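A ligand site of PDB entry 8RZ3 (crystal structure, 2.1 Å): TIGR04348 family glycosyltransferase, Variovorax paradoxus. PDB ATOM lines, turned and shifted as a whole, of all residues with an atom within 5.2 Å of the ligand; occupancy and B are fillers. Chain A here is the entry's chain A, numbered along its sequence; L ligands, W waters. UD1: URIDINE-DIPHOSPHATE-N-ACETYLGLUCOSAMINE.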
ATOM      1  N   ASN A  17     -21.266  11.409  -6.301  1.00  0.00           N
ATOM      2  CA  ASN A  17     -22.509  11.584  -5.563  1.00  0.00           C
ATOM      3  C   ASN A  17     -23.000  13.032  -5.696  1.00  0.00           C
ATOM      4  O   ASN A  17     -22.902  13.855  -4.791  1.00  0.00           O
ATOM      5  CB  ASN A  17     -22.309  11.169  -4.112  1.00  0.00           C
ATOM      6  CG  ASN A  17     -23.572  11.217  -3.284  1.00  0.00           C
ATOM      7  OD1 ASN A  17     -24.676  11.279  -3.824  1.00  0.00           O
ATOM      8  ND2 ASN A  17     -23.411  11.222  -1.968  1.00  0.00           N
ATOM      9  N   ASN A  18     -23.510  13.359  -6.886  1.00  0.00           N
ATOM     10  CA  ASN A  18     -24.000  14.694  -7.155  1.00  0.00           C
ATOM     11  C   ASN A  18     -25.132  14.629  -8.171  1.00  0.00           C
ATOM     12  O   ASN A  18     -25.437  13.573  -8.734  1.00  0.00           O
ATOM     13  CB  ASN A  18     -22.897  15.633  -7.668  1.00  0.00           C
ATOM     14  CG  ASN A  18     -22.277  15.172  -8.990  1.00  0.00           C
ATOM     15  OD1 ASN A  18     -22.941  14.592  -9.865  1.00  0.00           O
ATOM     16  ND2 ASN A  18     -20.982  15.436  -9.144  1.00  0.00           N
ATOM     17  N   GLY A  19     -25.717  15.809  -8.442  1.00  0.00           N
ATOM     18  CA  GLY A  19     -26.899  15.870  -9.283  1.00  0.00           C
ATOM     19  C   GLY A  19     -26.649  15.398 -10.703  1.00  0.00           C
ATOM     20  O   GLY A  19     -27.472  14.663 -11.263  1.00  0.00           O
ATOM     21  N   ASN A  20     -25.523  15.794 -11.297  1.00  0.00           N
ATOM     22  CA  ASN A  20     -25.284  15.473 -12.714  1.00  0.00           C
ATOM     23  C   ASN A  20     -25.162  13.979 -12.922  1.00  0.00           C
ATOM     24  O   ASN A  20     -25.777  13.416 -13.846  1.00  0.00           O
ATOM     25  CB  ASN A  20     -24.047  16.194 -13.228  1.00  0.00           C
ATOM     26  CG  ASN A  20     -24.340  17.606 -13.616  1.00  0.00           C
ATOM     27  OD1 ASN A  20     -25.495  18.011 -13.708  1.00  0.00           O
ATOM     28  ND2 ASN A  20     -23.301  18.374 -13.876  1.00  0.00           N
ATOM     29  N   ARG A  22     -26.422  11.694 -10.936  1.00  0.00           N
ATOM     30  CA  ARG A  22     -27.688  11.052 -10.559  1.00  0.00           C
ATOM     31  C   ARG A  22     -28.700  11.128 -11.688  1.00  0.00           C
ATOM     32  O   ARG A  22     -29.367  10.138 -12.015  1.00  0.00           O
ATOM     33  CB  ARG A  22     -28.215  11.707  -9.279  1.00  0.00           C
ATOM     34  CG  ARG A  22     -29.488  11.079  -8.731  1.00  0.00           C
ATOM     35  CD  ARG A  22     -29.505  11.129  -7.198  1.00  0.00           C
ATOM     36  NE  ARG A  22     -28.566  10.175  -6.634  1.00  0.00           N
ATOM     37  CZ  ARG A  22     -27.489  10.497  -5.927  1.00  0.00           C
ATOM     38  NH1 ARG A  22     -27.206  11.759  -5.631  1.00  0.00           N
ATOM     39  NH2 ARG A  22     -26.664   9.537  -5.515  1.00  0.00           N
ATOM     40  N   THR A  23     -28.831  12.306 -12.309  1.00  0.00           N
ATOM     41  CA  THR A  23     -29.700  12.454 -13.464  1.00  0.00           C
ATOM     42  C   THR A  23     -29.364  11.452 -14.555  1.00  0.00           C
ATOM     43  O   THR A  23     -30.235  10.711 -15.036  1.00  0.00           O
ATOM     44  CB  THR A  23     -29.599  13.870 -14.003  1.00  0.00           C
ATOM     45  OG1 THR A  23     -30.112  14.760 -13.012  1.00  0.00           O
ATOM     46  CG2 THR A  23     -30.374  14.000 -15.317  1.00  0.00           C
ATOM     47  N   LEU A  57     -25.769  16.887 -20.927  1.00  0.00           N
ATOM     48  CA  LEU A  57     -26.065  17.658 -19.734  1.00  0.00           C
ATOM     49  C   LEU A  57     -25.138  18.859 -19.651  1.00  0.00           C
ATOM     50  O   LEU A  57     -23.908  18.718 -19.732  1.00  0.00           O
ATOM     51  CB  LEU A  57     -25.933  16.803 -18.471  1.00  0.00           C
ATOM     52  CG  LEU A  57     -27.025  15.757 -18.257  1.00  0.00           C
ATOM     53  CD1 LEU A  57     -26.642  14.754 -17.194  1.00  0.00           C
ATOM     54  CD2 LEU A  57     -28.280  16.447 -17.843  1.00  0.00           C
ATOM     55  N   THR A  83     -29.080  22.249 -16.999  1.00  0.00           N
ATOM     56  CA  THR A  83     -28.957  21.808 -15.618  1.00  0.00           C
ATOM     57  C   THR A  83     -28.970  22.860 -14.550  1.00  0.00           C
ATOM     58  O   THR A  83     -29.056  22.526 -13.405  1.00  0.00           O
ATOM     59  CB  THR A  83     -27.746  20.901 -15.418  1.00  0.00           C
ATOM     60  OG1 THR A  83     -26.631  21.426 -16.103  1.00  0.00           O
ATOM     61  CG2 THR A  83     -28.013  19.573 -15.972  1.00  0.00           C
ATOM     62  N   GLY A  84     -28.898  24.121 -14.922  1.00  0.00           N
ATOM     63  CA  GLY A  84     -28.981  25.206 -13.978  1.00  0.00           C
ATOM     64  C   GLY A  84     -28.160  26.436 -14.282  1.00  0.00           C
ATOM     65  O   GLY A  84     -28.600  27.475 -14.663  1.00  0.00           O
ATOM     66  N   THR A  85     -26.917  26.249 -14.061  1.00  0.00           N
ATOM     67  CA  THR A  85     -25.905  27.270 -14.259  1.00  0.00           C
ATOM     68  C   THR A  85     -25.698  27.672 -15.686  1.00  0.00           C
ATOM     69  O   THR A  85     -25.202  28.741 -15.955  1.00  0.00           O
ATOM     70  CB  THR A  85     -24.534  26.964 -13.627  1.00  0.00           C
ATOM     71  OG1 THR A  85     -23.927  25.855 -14.260  1.00  0.00           O
ATOM     72  CG2 THR A  85     -24.638  26.707 -12.171  1.00  0.00           C
ATOM     73  N   LEU A 110     -35.694  21.553 -16.444  1.00  0.00           N
ATOM     74  CA  LEU A 110     -36.026  20.601 -15.386  1.00  0.00           C
ATOM     75  C   LEU A 110     -37.125  21.102 -14.433  1.00  0.00           C
ATOM     76  O   LEU A 110     -37.406  20.436 -13.434  1.00  0.00           O
ATOM     77  CB  LEU A 110     -34.767  20.223 -14.602  1.00  0.00           C
ATOM     78  CG  LEU A 110     -33.547  19.867 -15.469  1.00  0.00           C
ATOM     79  CD1 LEU A 110     -32.284  19.721 -14.623  1.00  0.00           C
ATOM     80  CD2 LEU A 110     -33.812  18.604 -16.287  1.00  0.00           C
ATOM     81  N   GLN A 131     -37.749  16.100 -12.782  1.00  0.00           N
ATOM     82  CA  GLN A 131     -37.019  14.935 -12.329  1.00  0.00           C
ATOM     83  C   GLN A 131     -37.856  14.130 -11.325  1.00  0.00           C
ATOM     84  O   GLN A 131     -38.903  14.569 -10.842  1.00  0.00           O
ATOM     85  CB  GLN A 131     -35.691  15.361 -11.746  1.00  0.00           C
ATOM     86  CG  GLN A 131     -34.971  16.406 -12.606  1.00  0.00           C
ATOM     87  CD  GLN A 131     -33.484  16.497 -12.340  1.00  0.00           C
ATOM     88  OE1 GLN A 131     -32.716  15.604 -12.720  1.00  0.00           O
ATOM     89  NE2 GLN A 131     -33.051  17.576 -11.714  1.00  0.00           N
ATOM     90  N   VAL A 151     -28.619  20.355   2.334  1.00  0.00           N
ATOM     91  CA  VAL A 151     -27.842  19.327   1.656  1.00  0.00           C
ATOM     92  C   VAL A 151     -27.339  19.915   0.352  1.00  0.00           C
ATOM     93  O   VAL A 151     -28.134  20.375  -0.480  1.00  0.00           O
ATOM     94  CB  VAL A 151     -28.682  18.067   1.366  1.00  0.00           C
ATOM     95  CG1 VAL A 151     -27.825  16.965   0.787  1.00  0.00           C
ATOM     96  CG2 VAL A 151     -29.488  17.655   2.612  1.00  0.00           C
ATOM     97  N   GLY A 152     -26.036  19.877   0.153  1.00  0.00           N
ATOM     98  CA  GLY A 152     -25.413  20.420  -1.033  1.00  0.00           C
ATOM     99  C   GLY A 152     -23.915  20.539  -0.833  1.00  0.00           C
ATOM    100  O   GLY A 152     -23.469  21.084   0.188  1.00  0.00           O
ATOM    101  N   HIS A 153     -23.138  19.996  -1.764  1.00  0.00           N
ATOM    102  CA  HIS A 153     -21.693  20.176  -1.705  1.00  0.00           C
ATOM    103  C   HIS A 153     -21.368  21.659  -1.771  1.00  0.00           C
ATOM    104  O   HIS A 153     -21.979  22.410  -2.548  1.00  0.00           O
ATOM    105  CB  HIS A 153     -21.035  19.396  -2.850  1.00  0.00           C
ATOM    106  CG  HIS A 153     -21.226  17.915  -2.765  1.00  0.00           C
ATOM    107  ND1 HIS A 153     -20.840  17.183  -1.650  1.00  0.00           N
ATOM    108  CD2 HIS A 153     -21.797  17.030  -3.619  1.00  0.00           C
ATOM    109  CE1 HIS A 153     -21.144  15.905  -1.844  1.00  0.00           C
ATOM    110  NE2 HIS A 153     -21.720  15.785  -3.023  1.00  0.00           N
ATOM    111  N   ARG A 155     -20.455  24.814  -2.769  1.00  0.00           N
ATOM    112  CA  ARG A 155     -20.025  25.630  -3.890  1.00  0.00           C
ATOM    113  C   ARG A 155     -20.723  26.965  -3.734  1.00  0.00           C
ATOM    114  O   ARG A 155     -21.814  27.028  -3.152  1.00  0.00           O
ATOM    115  CB  ARG A 155     -20.382  25.023  -5.268  1.00  0.00           C
ATOM    116  CG  ARG A 155     -19.778  23.660  -5.573  1.00  0.00           C
ATOM    117  CD  ARG A 155     -20.301  23.123  -6.927  1.00  0.00           C
ATOM    118  NE  ARG A 155     -20.707  21.725  -6.866  1.00  0.00           N
ATOM    119  CZ  ARG A 155     -19.947  20.703  -7.244  1.00  0.00           C
ATOM    120  NH1 ARG A 155     -18.719  20.885  -7.713  1.00  0.00           N
ATOM    121  NH2 ARG A 155     -20.439  19.460  -7.155  1.00  0.00           N
ATOM    122  N   VAL A 157     -22.441  28.630  -5.609  1.00  0.00           N
ATOM    123  CA  VAL A 157     -23.760  28.632  -6.247  1.00  0.00           C
ATOM    124  C   VAL A 157     -24.860  28.212  -5.283  1.00  0.00           C
ATOM    125  O   VAL A 157     -26.023  28.596  -5.457  1.00  0.00           O
ATOM    126  CB  VAL A 157     -23.696  27.743  -7.511  1.00  0.00           C
ATOM    127  CG1 VAL A 157     -25.048  27.607  -8.159  1.00  0.00           C
ATOM    128  CG2 VAL A 157     -22.682  28.258  -8.500  1.00  0.00           C
ATOM    129  N   LYS A 158     -24.514  27.441  -4.249  1.00  0.00           N
ATOM    130  CA  LYS A 158     -25.451  27.002  -3.233  1.00  0.00           C
ATOM    131  C   LYS A 158     -25.688  28.068  -2.176  1.00  0.00           C
ATOM    132  O   LYS A 158     -26.567  27.863  -1.316  1.00  0.00           O
ATOM    133  CB  LYS A 158     -24.962  25.725  -2.563  1.00  0.00           C
ATOM    134  CG  LYS A 158     -24.866  24.520  -3.479  1.00  0.00           C
ATOM    135  CD  LYS A 158     -26.216  24.135  -4.044  1.00  0.00           C
ATOM    136  CE  LYS A 158     -26.125  22.900  -5.000  1.00  0.00           C
ATOM    137  NZ  LYS A 158     -27.494  22.429  -5.411  1.00  0.00           N
ATOM    138  N   ILE A 181     -25.147  19.220   5.167  1.00  0.00           N
ATOM    139  CA  ILE A 181     -24.543  18.052   4.536  1.00  0.00           C
ATOM    140  C   ILE A 181     -23.977  18.465   3.201  1.00  0.00           C
ATOM    141  O   ILE A 181     -24.671  19.090   2.387  1.00  0.00           O
ATOM    142  CB  ILE A 181     -25.534  16.883   4.379  1.00  0.00           C
ATOM    143  CG1 ILE A 181     -26.091  16.460   5.743  1.00  0.00           C
ATOM    144  CG2 ILE A 181     -24.870  15.710   3.675  1.00  0.00           C
ATOM    145  CD1 ILE A 181     -27.263  15.442   5.615  1.00  0.00           C
ATOM    146  N   GLY A 182     -22.716  18.129   2.963  1.00  0.00           N
ATOM    147  CA  GLY A 182     -22.069  18.479   1.727  1.00  0.00           C
ATOM    148  C   GLY A 182     -20.578  18.518   1.887  1.00  0.00           C
ATOM    149  O   GLY A 182     -20.061  18.929   2.927  1.00  0.00           O
ATOM    150  N   ASP A 183     -19.876  18.107   0.833  1.00  0.00           N
ATOM    151  CA  ASP A 183     -18.430  18.135   0.797  1.00  0.00           C
ATOM    152  C   ASP A 183     -17.918  19.569   0.859  1.00  0.00           C
ATOM    153  O   ASP A 183     -18.646  20.526   0.552  1.00  0.00           O
ATOM    154  CB  ASP A 183     -17.960  17.432  -0.486  1.00  0.00           C
ATOM    155  CG  ASP A 183     -16.481  17.426  -0.638  1.00  0.00           C
ATOM    156  OD1 ASP A 183     -15.983  18.233  -1.456  1.00  0.00           O
ATOM    157  OD2 ASP A 183     -15.816  16.620   0.059  1.00  0.00           O
ATOM    158  N   GLY A 207     -20.136  17.342   6.733  1.00  0.00           N
ATOM    159  CA  GLY A 207     -19.357  16.886   5.601  1.00  0.00           C
ATOM    160  C   GLY A 207     -20.247  16.176   4.579  1.00  0.00           C
ATOM    161  O   GLY A 207     -21.478  16.246   4.607  1.00  0.00           O
ATOM    162  N   ALA A 208     -19.591  15.470   3.667  1.00  0.00           N
ATOM    163  CA  ALA A 208     -20.321  14.711   2.656  1.00  0.00           C
ATOM    164  C   ALA A 208     -20.840  13.409   3.249  1.00  0.00           C
ATOM    165  O   ALA A 208     -20.167  12.765   4.069  1.00  0.00           O
ATOM    166  CB  ALA A 208     -19.434  14.437   1.435  1.00  0.00           C
ATOM    167  N   LEU A 209     -22.042  13.029   2.846  1.00  0.00           N
ATOM    168  CA  LEU A 209     -22.639  11.810   3.349  1.00  0.00           C
ATOM    169  C   LEU A 209     -23.167  10.977   2.197  1.00  0.00           C
ATOM    170  O   LEU A 209     -23.745  11.523   1.240  1.00  0.00           O
ATOM    171  CB  LEU A 209     -23.771  12.114   4.334  1.00  0.00           C
ATOM    172  CG  LEU A 209     -23.387  12.798   5.650  1.00  0.00           C
ATOM    173  CD1 LEU A 209     -24.596  12.914   6.566  1.00  0.00           C
ATOM    174  CD2 LEU A 209     -22.250  12.055   6.327  1.00  0.00           C
ATOM    175  N   PRO A 210     -23.008   9.657   2.260  1.00  0.00           N
ATOM    176  CA  PRO A 210     -23.516   8.793   1.175  1.00  0.00           C
ATOM    177  C   PRO A 210     -25.004   8.965   1.014  1.00  0.00           C
ATOM    178  O   PRO A 210     -25.727   9.344   1.948  1.00  0.00           O
ATOM    179  CB  PRO A 210     -23.158   7.379   1.636  1.00  0.00           C
ATOM    180  CG  PRO A 210     -22.173   7.535   2.764  1.00  0.00           C
ATOM    181  CD  PRO A 210     -22.267   8.923   3.300  1.00  0.00           C
ATOM    182  N   HIS A 211     -25.476   8.688  -0.199  1.00  0.00           N
ATOM    183  CA  HIS A 211     -26.811   9.138  -0.590  1.00  0.00           C
ATOM    184  C   HIS A 211     -27.889   8.555   0.315  1.00  0.00           C
ATOM    185  O   HIS A 211     -28.871   9.238   0.629  1.00  0.00           O
ATOM    186  CB  HIS A 211     -27.103   8.786  -2.041  1.00  0.00           C
ATOM    187  CG  HIS A 211     -28.348   9.418  -2.546  1.00  0.00           C
ATOM    188  ND1 HIS A 211     -29.449   8.692  -2.929  1.00  0.00           N
ATOM    189  CD2 HIS A 211     -28.686  10.717  -2.666  1.00  0.00           C
ATOM    190  CE1 HIS A 211     -30.415   9.521  -3.295  1.00  0.00           C
ATOM    191  NE2 HIS A 211     -29.977  10.762  -3.134  1.00  0.00           N
ATOM    192  N   THR A 214     -28.018  10.407   3.559  1.00  0.00           N
ATOM    193  CA  THR A 214     -28.495  11.761   3.295  1.00  0.00           C
ATOM    194  C   THR A 214     -30.012  11.806   3.197  1.00  0.00           C
ATOM    195  O   THR A 214     -30.654  12.694   3.767  1.00  0.00           O
ATOM    196  CB  THR A 214     -27.870  12.272   1.993  1.00  0.00           C
ATOM    197  OG1 THR A 214     -26.459  12.466   2.169  1.00  0.00           O
ATOM    198  CG2 THR A 214     -28.516  13.583   1.575  1.00  0.00           C
ATOM    199  N   ILE A 218     -32.707  13.776   5.552  1.00  0.00           N
ATOM    200  CA  ILE A 218     -33.746  14.646   4.990  1.00  0.00           C
ATOM    201  C   ILE A 218     -35.110  14.233   5.504  1.00  0.00           C
ATOM    202  O   ILE A 218     -35.920  15.058   5.930  1.00  0.00           O
ATOM    203  CB  ILE A 218     -33.689  14.614   3.444  1.00  0.00           C
ATOM    204  CG1 ILE A 218     -32.455  15.355   2.919  1.00  0.00           C
ATOM    205  CG2 ILE A 218     -34.911  15.212   2.826  1.00  0.00           C
ATOM    206  CD1 ILE A 218     -32.163  15.061   1.464  1.00  0.00           C
ATOM    207  N   HIS A 226     -32.872  25.403   1.655  1.00  0.00           N
ATOM    208  CA  HIS A 226     -32.124  25.417   0.407  1.00  0.00           C
ATOM    209  C   HIS A 226     -32.015  26.864  -0.083  1.00  0.00           C
ATOM    210  O   HIS A 226     -33.028  27.465  -0.485  1.00  0.00           O
ATOM    211  CB  HIS A 226     -32.767  24.522  -0.634  1.00  0.00           C
ATOM    212  CG  HIS A 226     -31.839  24.128  -1.741  1.00  0.00           C
ATOM    213  ND1 HIS A 226     -30.715  23.346  -1.544  1.00  0.00           N
ATOM    214  CD2 HIS A 226     -31.833  24.443  -3.060  1.00  0.00           C
ATOM    215  CE1 HIS A 226     -30.095  23.169  -2.697  1.00  0.00           C
ATOM    216  NE2 HIS A 226     -30.738  23.839  -3.622  1.00  0.00           N
ATOM    217  N   LEU A 230     -29.143  29.701  -7.732  1.00  0.00           N
ATOM    218  CA  LEU A 230     -29.811  29.256  -8.933  1.00  0.00           C
ATOM    219  C   LEU A 230     -29.787  27.732  -8.920  1.00  0.00           C
ATOM    220  O   LEU A 230     -28.872  27.129  -8.369  1.00  0.00           O
ATOM    221  CB  LEU A 230     -29.134  29.794 -10.210  1.00  0.00           C
ATOM    222  CG  LEU A 230     -27.639  29.496 -10.357  1.00  0.00           C
ATOM    223  CD1 LEU A 230     -27.387  28.117 -10.988  1.00  0.00           C
ATOM    224  CD2 LEU A 230     -26.964  30.584 -11.170  1.00  0.00           C
ATOM    225  N   GLU A 231     -30.807  27.137  -9.530  1.00  0.00           N
ATOM    226  CA  GLU A 231     -30.958  25.692  -9.585  1.00  0.00           C
ATOM    227  C   GLU A 231     -31.619  25.324 -10.904  1.00  0.00           C
ATOM    228  O   GLU A 231     -32.529  26.008 -11.362  1.00  0.00           O
ATOM    229  CB  GLU A 231     -31.822  25.162  -8.425  1.00  0.00           C
ATOM    230  CG  GLU A 231     -31.123  25.158  -7.076  1.00  0.00           C
ATOM    231  CD  GLU A 231     -30.052  24.098  -6.956  1.00  0.00           C
ATOM    232  OE1 GLU A 231     -29.980  23.215  -7.844  1.00  0.00           O
ATOM    233  OE2 GLU A 231     -29.258  24.141  -5.997  1.00  0.00           O
ATOM    234  N   GLY A 232     -31.133  24.253 -11.528  1.00  0.00           N
ATOM    235  CA  GLY A 232     -31.900  23.734 -12.633  1.00  0.00           C
ATOM    236  C   GLY A 232     -33.207  23.106 -12.190  1.00  0.00           C
ATOM    237  O   GLY A 232     -34.145  23.003 -12.996  1.00  0.00           O
ATOM    238  N   GLY A 233     -33.309  22.715 -10.924  1.00  0.00           N
ATOM    239  CA  GLY A 233     -34.322  21.800 -10.431  1.00  0.00           C
ATOM    240  C   GLY A 233     -33.629  20.837  -9.491  1.00  0.00           C
ATOM    241  O   GLY A 233     -33.312  19.709  -9.880  1.00  0.00           O
ATOM    242  N   ALA A 234     -33.382  21.277  -8.256  1.00  0.00           N
ATOM    243  CA  ALA A 234     -32.497  20.573  -7.327  1.00  0.00           C
ATOM    244  C   ALA A 234     -33.053  19.220  -6.900  1.00  0.00           C
ATOM    245  O   ALA A 234     -34.217  19.114  -6.473  1.00  0.00           O
ATOM    246  CB  ALA A 234     -32.255  21.434  -6.090  1.00  0.00           C
ATOM    247  N   HIS A 235     -32.206  18.189  -6.949  1.00  0.00           N
ATOM    248  CA  HIS A 235     -32.591  16.889  -6.431  1.00  0.00           C
ATOM    249  C   HIS A 235     -33.022  16.961  -4.972  1.00  0.00           C
ATOM    250  O   HIS A 235     -33.977  16.291  -4.572  1.00  0.00           O
ATOM    251  CB  HIS A 235     -31.440  15.899  -6.559  1.00  0.00           C
ATOM    252  CG  HIS A 235     -31.354  15.238  -7.893  1.00  0.00           C
ATOM    253  ND1 HIS A 235     -30.609  15.757  -8.930  1.00  0.00           N
ATOM    254  CD2 HIS A 235     -31.896  14.088  -8.356  1.00  0.00           C
ATOM    255  CE1 HIS A 235     -30.720  14.972  -9.978  1.00  0.00           C
ATOM    256  NE2 HIS A 235     -31.492  13.950  -9.659  1.00  0.00           N
ATOM    257  N   VAL A 236     -32.320  17.768  -4.151  1.00  0.00           N
ATOM    258  CA  VAL A 236     -32.533  17.717  -2.711  1.00  0.00           C
ATOM    259  C   VAL A 236     -33.952  18.175  -2.368  1.00  0.00           C
ATOM    260  O   VAL A 236     -34.542  17.716  -1.383  1.00  0.00           O
ATOM    261  CB  VAL A 236     -31.460  18.522  -1.950  1.00  0.00           C
ATOM    262  CG1 VAL A 236     -30.082  17.900  -2.132  1.00  0.00           C
ATOM    263  CG2 VAL A 236     -31.451  19.986  -2.395  1.00  0.00           C
ATOM    264  N   GLU A 239     -36.339  15.313  -3.042  1.00  0.00           N
ATOM    265  CA  GLU A 239     -36.082  14.255  -2.063  1.00  0.00           C
ATOM    266  C   GLU A 239     -36.781  14.559  -0.758  1.00  0.00           C
ATOM    267  O   GLU A 239     -37.325  13.661  -0.093  1.00  0.00           O
ATOM    268  CB  GLU A 239     -34.571  14.102  -1.868  1.00  0.00           C
ATOM    269  CG  GLU A 239     -33.866  13.399  -3.049  1.00  0.00           C
ATOM    270  CD  GLU A 239     -32.367  13.595  -3.018  1.00  0.00           C
ATOM    271  OE1 GLU A 239     -31.846  14.175  -2.032  1.00  0.00           O
ATOM    272  OE2 GLU A 239     -31.704  13.168  -3.996  1.00  0.00           O
HETATM  273  C1' UD1 L   1     -27.103  20.077 -10.448  1.00  0.00           C
HETATM  274  C2' UD1 L   1     -28.097  21.206 -10.415  1.00  0.00           C
HETATM  275  C3' UD1 L   1     -29.437  20.606 -10.172  1.00  0.00           C
HETATM  276  C4' UD1 L   1     -29.828  19.735 -11.285  1.00  0.00           C
HETATM  277  C5' UD1 L   1     -28.762  18.698 -11.564  1.00  0.00           C
HETATM  278  C6' UD1 L   1     -29.076  18.060 -12.871  1.00  0.00           C
HETATM  279  C7' UD1 L   1     -27.580  23.596  -9.628  1.00  0.00           C
HETATM  280  C8' UD1 L   1     -27.842  24.054 -11.079  1.00  0.00           C
HETATM  281  N2' UD1 L   1     -27.697  22.166  -9.325  1.00  0.00           N
HETATM  282  O1' UD1 L   1     -27.310  19.279  -9.295  1.00  0.00           O
HETATM  283  O3' UD1 L   1     -30.476  21.619 -10.028  1.00  0.00           O
HETATM  284  O4' UD1 L   1     -31.062  19.051 -10.929  1.00  0.00           O
HETATM  285  O5' UD1 L   1     -27.401  19.291 -11.614  1.00  0.00           O
HETATM  286  O6' UD1 L   1     -28.156  17.032 -13.081  1.00  0.00           O
HETATM  287  O7' UD1 L   1     -27.280  24.406  -8.811  1.00  0.00           O
HETATM  288  N1  UD1 L   1     -25.863  14.397  -1.979  1.00  0.00           N
HETATM  289  C2  UD1 L   1     -25.590  13.288  -1.005  1.00  0.00           C
HETATM  290  N3  UD1 L   1     -24.552  13.650   0.084  1.00  0.00           N
HETATM  291  C4  UD1 L   1     -23.921  14.947   0.118  1.00  0.00           C
HETATM  292  C5  UD1 L   1     -24.222  15.958  -0.857  1.00  0.00           C
HETATM  293  C6  UD1 L   1     -25.191  15.682  -1.917  1.00  0.00           C
HETATM  294  O2  UD1 L   1     -26.143  12.236  -1.074  1.00  0.00           O
HETATM  295  O4  UD1 L   1     -23.135  15.169   0.953  1.00  0.00           O
HETATM  296  C1B UD1 L   1     -26.823  14.111  -3.041  1.00  0.00           C
HETATM  297  C2B UD1 L   1     -28.168  14.862  -2.849  1.00  0.00           C
HETATM  298  O2' UD1 L   1     -29.061  14.114  -2.184  1.00  0.00           O
HETATM  299  C3B UD1 L   1     -28.640  15.011  -4.336  1.00  0.00           C
HETATM  300  C4B UD1 L   1     -27.554  15.197  -5.011  1.00  0.00           C
HETATM  301  O4B UD1 L   1     -26.299  14.581  -4.130  1.00  0.00           O
HETATM  302  O3B UD1 L   1     -29.284  13.748  -4.733  1.00  0.00           O
HETATM  303  C5B UD1 L   1     -27.299  16.671  -5.222  1.00  0.00           C
HETATM  304  O5B UD1 L   1     -28.114  16.986  -6.374  1.00  0.00           O
HETATM  305  PA  UD1 L   1     -28.718  18.501  -6.480  1.00  0.00           P
HETATM  306  O1A UD1 L   1     -29.550  18.575  -7.732  1.00  0.00           O
HETATM  307  O2A UD1 L   1     -29.516  18.850  -5.258  1.00  0.00           O
HETATM  308  O3A UD1 L   1     -27.417  19.548  -6.542  1.00  0.00           O
HETATM  309  PB  UD1 L   1     -26.435  19.537  -7.878  1.00  0.00           P
HETATM  310  O1B UD1 L   1     -25.482  18.414  -7.688  1.00  0.00           O
HETATM  311  O2B UD1 L   1     -25.807  20.893  -7.897  1.00  0.00           O
HETATM  312  O   HOH W   1     -24.116  18.102 -10.036  1.00  0.00           O
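O of Leu 230 lies close to O7' of the ligand (3.2 Å). Residues that only touch the ligand: Thr 83, His 153, Ile 181, Ala 208, Gly 84, Gly 182, Asn 18, Thr 85, Leu 110, Val 157 and Val 151. Hydrophobic or aromatic side chains within 4 Å of the ligand: Leu 110, Val 151, His 153, Val 157, Ile 181, Ala 208, His 211, Ala 234, His 235 and Val 236. 29 residues have an atom within 4 Å of the ligand: Asn 17, Asn 18, Gly 19, Asn 20, Arg 22, Thr 23, Thr 83, Gly 84, Thr 85, Leu 110, Gln 131, Val 151, His 153, Val 157, Lys 158, Ile 181, Gly 182, Ala 208, Leu 209, His 211, Thr 214, Leu 230, Glu 231, Gly 232, Gly 233, Ala 234, His 235, Val 236 and Glu 239.
Water W1 lies within hydrogen-bond range of an oxygen (O1B) of the ligand (2.7 Å), the backbone NH (N) of Asn 20 (3.0 Å) and the backbone NH (N) of Gly 19 (3.2 Å).
The backbone carbonyl oxygen (O) of Leu 209 is in hydrogen-bond range of the side-chain amide nitrogen (ND2) of Asn 17, 3.2 Å away. OE2 of Glu 239 sits at hydrogen-bond distance from NE2 of His 211. O of Gly 19 sits at hydrogen-bond distance from OG1 of Thr 23. The side-chain carboxylate (OE2) of Glu 231 is in salt-bridge range of the side-chain amino group (NZ) of Lys 158, 2.5 Å away. NE2 of His 226 is in hydrogen-bond range of OE2 of Glu 231, at 2.8 Å. OD1 of Asn 18 sits at hydrogen-bond distance from N of Asn 20, 3.2 Å away. The backbone carbonyl oxygen (O) of Thr 83 sits close to the backbone NH (N) of Gly 232 (3.3 Å). ND1 of His 153 sits at hydrogen-bond distance from N of Asp 183.
The backbone NH of Leu 209 is in hydrogen-bond range of an oxygen (O4) of the ligand (3.1 Å). The backbone carbonyl oxygen (O) of Leu 209 lies within hydrogen-bond range of a nitrogen (N3) of the ligand (2.6 Å). N of Gly 233 is in hydrogen-bond range of O3' of the ligand (3.2 Å). O4' of the ligand is in hydrogen-bond range of O of Gly 233 (2.6 Å). The side-chain carboxylate of Glu 239 is in hydrogen-bond range of an oxygen (O3B) of the ligand (2.6 Å). The side-chain amide nitrogen (NE2) of Gln 131 lies within hydrogen-bond range of an oxygen (O4') of the ligand, at 2.6 Å. O1B of the ligand lies within hydrogen-bond range of N of Gly 19 (2.7 Å). An oxygen (O6') of the ligand is in hydrogen-bond range of the backbone carbonyl oxygen (O) of Gly 19 (3.1 Å). OE1 of Glu 231 sits at hydrogen-bond distance from O3' of the ligand. N of His 235 is in hydrogen-bond range of O1A of the ligand, 2.8 Å away. A ring nitrogen (ND1) of His 235 sits at hydrogen-bond distance from an oxygen (O1A) of the ligand (3.2 Å). N of Asn 20 lies close to O6' of the ligand. The side-chain amide oxygen of Asn 20 sits at hydrogen-bond distance from an oxygen (O6') of the ligand (2.9 Å). The side-chain hydroxyl (OG1) of Thr 23 is in hydrogen-bond range of an oxygen (O6') of the ligand (3.0 Å). NH1 of Arg 22 lies within hydrogen-bond range of O3B of the ligand, at 3.0 Å. ND2 of Asn 17 is in hydrogen-bond range of O2 of the ligand, 3.0 Å away. The side-chain hydroxyl of Thr 214 lies within hydrogen-bond range of a nitrogen (N3) of the ligand (3.1 Å). The side-chain amino group (NZ) of Lys 158 is in salt-bridge range of an oxygen (O2B) of the ligand, at 3.4 Å. N of Gly 232 is in hydrogen-bond range of O3' of the ligand, 3.1 Å away. The backbone NH (N) of Val 236 lies within hydrogen-bond range of an oxygen (O2A) of the ligand. A ring nitrogen (NE2) of His 211 sits at hydrogen-bond distance from an oxygen (O3B) of the ligand (3.5 Å). O3' of the ligand is in hydrogen-bond range of N of Ala 234.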
